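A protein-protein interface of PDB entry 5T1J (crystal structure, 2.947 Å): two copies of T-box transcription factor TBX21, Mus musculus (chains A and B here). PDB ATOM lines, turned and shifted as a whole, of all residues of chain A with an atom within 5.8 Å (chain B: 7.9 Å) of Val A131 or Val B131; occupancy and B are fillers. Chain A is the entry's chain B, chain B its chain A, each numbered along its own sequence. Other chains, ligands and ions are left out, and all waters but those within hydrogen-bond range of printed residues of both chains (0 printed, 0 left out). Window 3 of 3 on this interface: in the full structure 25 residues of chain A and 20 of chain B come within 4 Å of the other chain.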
ATOM      1  N   ALA A 127      32.828 -16.049   5.791  1.00  0.00           N
ATOM      2  CA  ALA A 127      33.409 -15.715   4.489  1.00  0.00           C
ATOM      3  C   ALA A 127      32.815 -14.472   3.848  1.00  0.00           C
ATOM      4  O   ALA A 127      32.488 -14.478   2.663  1.00  0.00           O
ATOM      5  CB  ALA A 127      33.295 -16.903   3.539  1.00  0.00           C
ATOM      6  N   SER A 128      32.647 -13.432   4.657  1.00  0.00           N
ATOM      7  CA  SER A 128      32.373 -12.096   4.154  1.00  0.00           C
ATOM      8  C   SER A 128      30.980 -11.989   3.489  1.00  0.00           C
ATOM      9  O   SER A 128      30.831 -11.491   2.370  1.00  0.00           O
ATOM     10  CB  SER A 128      33.501 -11.687   3.188  1.00  0.00           C
ATOM     11  OG  SER A 128      34.753 -12.141   3.688  1.00  0.00           O
ATOM     12  N   ASN A 129      29.969 -12.371   4.280  1.00  0.00           N
ATOM     13  CA  ASN A 129      28.551 -12.538   3.938  1.00  0.00           C
ATOM     14  C   ASN A 129      28.408 -13.367   2.669  1.00  0.00           C
ATOM     15  O   ASN A 129      27.522 -13.120   1.848  1.00  0.00           O
ATOM     16  CB  ASN A 129      27.725 -11.226   3.792  1.00  0.00           C
ATOM     17  CG  ASN A 129      28.375  -9.997   4.400  1.00  0.00           C
ATOM     18  OD1 ASN A 129      27.680  -9.073   4.889  1.00  0.00           O
ATOM     19  ND2 ASN A 129      29.674  -9.841   4.130  1.00  0.00           N
ATOM     20  N   ASN A 130      29.341 -14.299   2.504  1.00  0.00           N
ATOM     21  CA  ASN A 130      29.642 -15.042   1.273  1.00  0.00           C
ATOM     22  C   ASN A 130      30.075 -14.136   0.077  1.00  0.00           C
ATOM     23  O   ASN A 130      31.107 -13.454   0.206  1.00  0.00           O
ATOM     24  CB  ASN A 130      28.444 -15.963   0.984  1.00  0.00           C
ATOM     25  CG  ASN A 130      28.470 -16.568  -0.403  1.00  0.00           C
ATOM     26  OD1 ASN A 130      27.991 -15.953  -1.359  1.00  0.00           O
ATOM     27  ND2 ASN A 130      29.107 -17.733  -0.538  1.00  0.00           N
ATOM     28  N   VAL A 131      29.329 -14.056  -1.029  1.00  0.00           N
ATOM     29  CA  VAL A 131      29.915 -13.671  -2.331  1.00  0.00           C
ATOM     30  C   VAL A 131      31.291 -14.400  -2.425  1.00  0.00           C
ATOM     31  O   VAL A 131      32.357 -13.788  -2.530  1.00  0.00           O
ATOM     32  CB  VAL A 131      29.975 -12.087  -2.464  1.00  0.00           C
ATOM     33  CG1 VAL A 131      31.067 -11.523  -3.403  1.00  0.00           C
ATOM     34  CG2 VAL A 131      28.581 -11.493  -2.712  1.00  0.00           C
ATOM     35  N   THR A 132      31.248 -15.737  -2.317  1.00  0.00           N
ATOM     36  CA  THR A 132      32.459 -16.584  -2.376  1.00  0.00           C
ATOM     37  C   THR A 132      32.333 -17.799  -3.310  1.00  0.00           C
ATOM     38  O   THR A 132      32.944 -17.824  -4.373  1.00  0.00           O
ATOM     39  CB  THR A 132      32.872 -17.111  -0.953  1.00  0.00           C
ATOM     40  OG1 THR A 132      31.934 -18.088  -0.461  1.00  0.00           O
ATOM     41  CG2 THR A 132      33.021 -15.975   0.035  1.00  0.00           C
ATOM     42  N   GLN A 133      31.516 -18.776  -2.910  1.00  0.00           N
ATOM     43  CA  GLN A 133      31.376 -20.073  -3.591  1.00  0.00           C
ATOM     44  C   GLN A 133      32.747 -20.748  -3.638  1.00  0.00           C
ATOM     45  O   GLN A 133      33.265 -21.177  -4.687  1.00  0.00           O
ATOM     46  CB  GLN A 133      30.775 -19.942  -4.989  1.00  0.00           C
ATOM     47  CG  GLN A 133      30.435 -21.291  -5.656  1.00  0.00           C
ATOM     48  CD  GLN A 133      29.804 -21.126  -7.032  1.00  0.00           C
ATOM     49  OE1 GLN A 133      29.142 -20.108  -7.313  1.00  0.00           O
ATOM     50  NE2 GLN A 133      30.016 -22.124  -7.909  1.00  0.00           N
ATOM     51  N   GLN B  39      22.884  -6.853 -10.377  1.00  0.00           N
ATOM     52  CA  GLN B  39      23.720  -6.873  -9.186  1.00  0.00           C
ATOM     53  C   GLN B  39      23.209  -7.943  -8.222  1.00  0.00           C
ATOM     54  O   GLN B  39      23.988  -8.665  -7.602  1.00  0.00           O
ATOM     55  CB  GLN B  39      23.772  -5.513  -8.476  1.00  0.00           C
ATOM     56  CG  GLN B  39      24.315  -5.682  -7.028  1.00  0.00           C
ATOM     57  CD  GLN B  39      24.484  -4.403  -6.220  1.00  0.00           C
ATOM     58  OE1 GLN B  39      23.647  -3.502  -6.267  1.00  0.00           O
ATOM     59  NE2 GLN B  39      25.583  -4.326  -5.465  1.00  0.00           N
ATOM     60  N   TYR B  97      21.758 -22.739  -3.151  1.00  0.00           N
ATOM     61  CA  TYR B  97      22.142 -21.815  -2.097  1.00  0.00           C
ATOM     62  C   TYR B  97      22.156 -22.504  -0.745  1.00  0.00           C
ATOM     63  O   TYR B  97      21.064 -22.646  -0.119  1.00  0.00           O
ATOM     64  CB  TYR B  97      21.196 -20.622  -2.027  1.00  0.00           C
ATOM     65  CG  TYR B  97      21.683 -19.502  -1.128  1.00  0.00           C
ATOM     66  CD1 TYR B  97      22.390 -18.426  -1.651  1.00  0.00           C
ATOM     67  CD2 TYR B  97      21.429 -19.522   0.247  1.00  0.00           C
ATOM     68  CE1 TYR B  97      22.821 -17.399  -0.837  1.00  0.00           C
ATOM     69  CE2 TYR B  97      21.861 -18.503   1.069  1.00  0.00           C
ATOM     70  CZ  TYR B  97      22.559 -17.442   0.523  1.00  0.00           C
ATOM     71  OH  TYR B  97      22.997 -16.415   1.322  1.00  0.00           O
ATOM     72  N   LYS B 120      20.494 -13.903  -2.753  1.00  0.00           N
ATOM     73  CA  LYS B 120      20.151 -12.891  -3.757  1.00  0.00           C
ATOM     74  C   LYS B 120      19.767 -13.572  -5.067  1.00  0.00           C
ATOM     75  O   LYS B 120      20.283 -14.690  -5.357  1.00  0.00           O
ATOM     76  CB  LYS B 120      21.284 -11.907  -4.056  1.00  0.00           C
ATOM     77  CG  LYS B 120      21.999 -11.321  -2.903  1.00  0.00           C
ATOM     78  CD  LYS B 120      21.244 -10.310  -2.163  1.00  0.00           C
ATOM     79  CE  LYS B 120      22.189  -9.234  -1.685  1.00  0.00           C
ATOM     80  NZ  LYS B 120      22.768  -8.517  -2.869  1.00  0.00           N
ATOM     81  N   ALA B 127      28.464 -15.186 -14.284  1.00  0.00           N
ATOM     82  CA  ALA B 127      28.409 -14.536 -12.976  1.00  0.00           C
ATOM     83  C   ALA B 127      29.782 -14.239 -12.408  1.00  0.00           C
ATOM     84  O   ALA B 127      30.019 -14.471 -11.217  1.00  0.00           O
ATOM     85  CB  ALA B 127      27.617 -15.404 -11.989  1.00  0.00           C
ATOM     86  N   SER B 128      30.682 -13.762 -13.266  1.00  0.00           N
ATOM     87  CA  SER B 128      31.958 -13.220 -12.816  1.00  0.00           C
ATOM     88  C   SER B 128      32.810 -14.311 -12.198  1.00  0.00           C
ATOM     89  O   SER B 128      33.185 -14.192 -11.039  1.00  0.00           O
ATOM     90  CB  SER B 128      31.750 -12.084 -11.802  1.00  0.00           C
ATOM     91  OG  SER B 128      32.939 -11.331 -11.621  1.00  0.00           O
ATOM     92  N   ASN B 129      33.084 -15.366 -12.969  1.00  0.00           N
ATOM     93  CA  ASN B 129      33.707 -16.615 -12.495  1.00  0.00           C
ATOM     94  C   ASN B 129      33.280 -17.066 -11.091  1.00  0.00           C
ATOM     95  O   ASN B 129      34.091 -17.561 -10.319  1.00  0.00           O
ATOM     96  CB  ASN B 129      35.243 -16.519 -12.596  1.00  0.00           C
ATOM     97  CG  ASN B 129      35.847 -15.400 -11.749  1.00  0.00           C
ATOM     98  OD1 ASN B 129      35.420 -15.135 -10.629  1.00  0.00           O
ATOM     99  ND2 ASN B 129      36.861 -14.738 -12.297  1.00  0.00           N
ATOM    100  N   ASN B 130      31.982 -16.943 -10.819  1.00  0.00           N
ATOM    101  CA  ASN B 130      31.357 -16.974  -9.483  1.00  0.00           C
ATOM    102  C   ASN B 130      31.864 -15.892  -8.512  1.00  0.00           C
ATOM    103  O   ASN B 130      31.717 -14.697  -8.797  1.00  0.00           O
ATOM    104  CB  ASN B 130      31.519 -18.377  -8.870  1.00  0.00           C
ATOM    105  CG  ASN B 130      31.161 -19.478  -9.859  1.00  0.00           C
ATOM    106  OD1 ASN B 130      30.498 -19.221 -10.838  1.00  0.00           O
ATOM    107  ND2 ASN B 130      31.626 -20.689  -9.622  1.00  0.00           N
ATOM    108  N   VAL B 131      32.479 -16.301  -7.403  1.00  0.00           N
ATOM    109  CA  VAL B 131      32.587 -15.469  -6.195  1.00  0.00           C
ATOM    110  C   VAL B 131      31.281 -14.684  -5.979  1.00  0.00           C
ATOM    111  O   VAL B 131      31.309 -13.469  -5.764  1.00  0.00           O
ATOM    112  CB  VAL B 131      33.801 -14.494  -6.318  1.00  0.00           C
ATOM    113  CG1 VAL B 131      34.029 -13.707  -5.043  1.00  0.00           C
ATOM    114  CG2 VAL B 131      35.062 -15.289  -6.525  1.00  0.00           C
ATOM    115  N   THR B 132      30.150 -15.407  -6.008  1.00  0.00           N
ATOM    116  CA  THR B 132      28.781 -14.855  -5.829  1.00  0.00           C
ATOM    117  C   THR B 132      27.902 -15.683  -4.876  1.00  0.00           C
ATOM    118  O   THR B 132      27.494 -15.200  -3.828  1.00  0.00           O
ATOM    119  CB  THR B 132      28.002 -14.701  -7.180  1.00  0.00           C
ATOM    120  OG1 THR B 132      27.798 -15.987  -7.795  1.00  0.00           O
ATOM    121  CG2 THR B 132      28.764 -13.811  -8.137  1.00  0.00           C
ATOM    122  N   GLN B 133      27.602 -16.919  -5.284  1.00  0.00           N
ATOM    123  CA  GLN B 133      26.666 -17.822  -4.601  1.00  0.00           C
ATOM    124  C   GLN B 133      25.275 -17.181  -4.538  1.00  0.00           C
ATOM    125  O   GLN B 133      24.643 -17.044  -3.471  1.00  0.00           O
ATOM    126  CB  GLN B 133      27.166 -18.232  -3.201  1.00  0.00           C
ATOM    127  CG  GLN B 133      26.297 -19.313  -2.468  1.00  0.00           C
ATOM    128  CD  GLN B 133      26.821 -19.711  -1.074  1.00  0.00           C
ATOM    129  OE1 GLN B 133      28.030 -19.661  -0.815  1.00  0.00           O
ATOM    130  NE2 GLN B 133      25.898 -20.054  -0.158  1.00  0.00           N
ATOM    131  N   MET B 134      24.758 -16.847  -5.714  1.00  0.00           N
ATOM    132  CA  MET B 134      23.435 -16.260  -5.765  1.00  0.00           C
ATOM    133  C   MET B 134      22.738 -16.853  -6.966  1.00  0.00           C
ATOM    134  O   MET B 134      23.359 -17.105  -7.997  1.00  0.00           O
ATOM    135  CB  MET B 134      23.519 -14.718  -5.788  1.00  0.00           C
ATOM    136  CG  MET B 134      24.244 -14.080  -6.960  1.00  0.00           C
ATOM    137  SD  MET B 134      24.555 -12.328  -6.599  1.00  0.00           S
ATOM    138  CE  MET B 134      25.364 -11.767  -8.097  1.00  0.00           C
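O of Thr B132 sits close to OD1 of Asn A130, 2.6 Å away. ND2 of Asn B130 sits close to NE2 of Gln A133, at 2.8 Å. O of Val A131 lies close to O of Val B131, 3.4 Å away. The side-chain amide nitrogen (ND2) of Asn A130 sits close to the side-chain amide oxygen (OE1) of Gln B133, at 2.2 Å. The backbone NH (N) of Val B131 sits close to the backbone carbonyl oxygen (O) of Thr A132 (3.4 Å).
The side-chain amide nitrogen of Asn A130 lies within hydrogen-bond range of the side-chain hydroxyl of Thr A132 (2.9 Å).
Among the printed residues, merely in contact across the chains: Val A131 with Thr B132 (3.2 Å) and Thr A132 with Thr B132 (3.9 Å).
Of the printed residues of chain B, Val A131 touches Val B131 and Thr B132. Of the printed residues of chain B, Thr A132 touches Val B131 (3.0 Å) and Thr B132 (3.9 Å). Printed residues of chain B within 4 Å of Gln A133: Asn B130. Printed residues of chain A within 4 Å of Asn B130: Gln A133 (2.8 Å). Val B131 touches just these residues of chain A: Val A131 (3.0 Å) and Thr A132 (3.0 Å). Printed residues of chain A within 4 Å of Thr B132: Asn A130, Val A131 and Thr A132. The nearest printed residue of chain A that does not touch Thr B132 is Gln A133 (4.4 Å).
Of the 7 printed residues of chain A, 4 touch a printed residue of chain B. Among the printed residues, no Asp or Glu carboxylate lies within 4 Å of a Lys or Arg side-chain nitrogen of the other chain.
Asn A130 touches Thr B132, but with the chains exchanged Thr A132 does not touch Asn B130 (4.7 Å). Asn A130 touches Gln B133, and with the chains exchanged Gln A133 touches Asn B130. Val A131 touches Thr B132, and with the chains exchanged Thr A132 touches Val B131. Thr B132 touches its own counterpart, Thr A132. 7 positions are printed for both chains. Of the 7 pairs that touch across the chains among the printed residues, 6 have their exchanged pair printed and touching as well.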
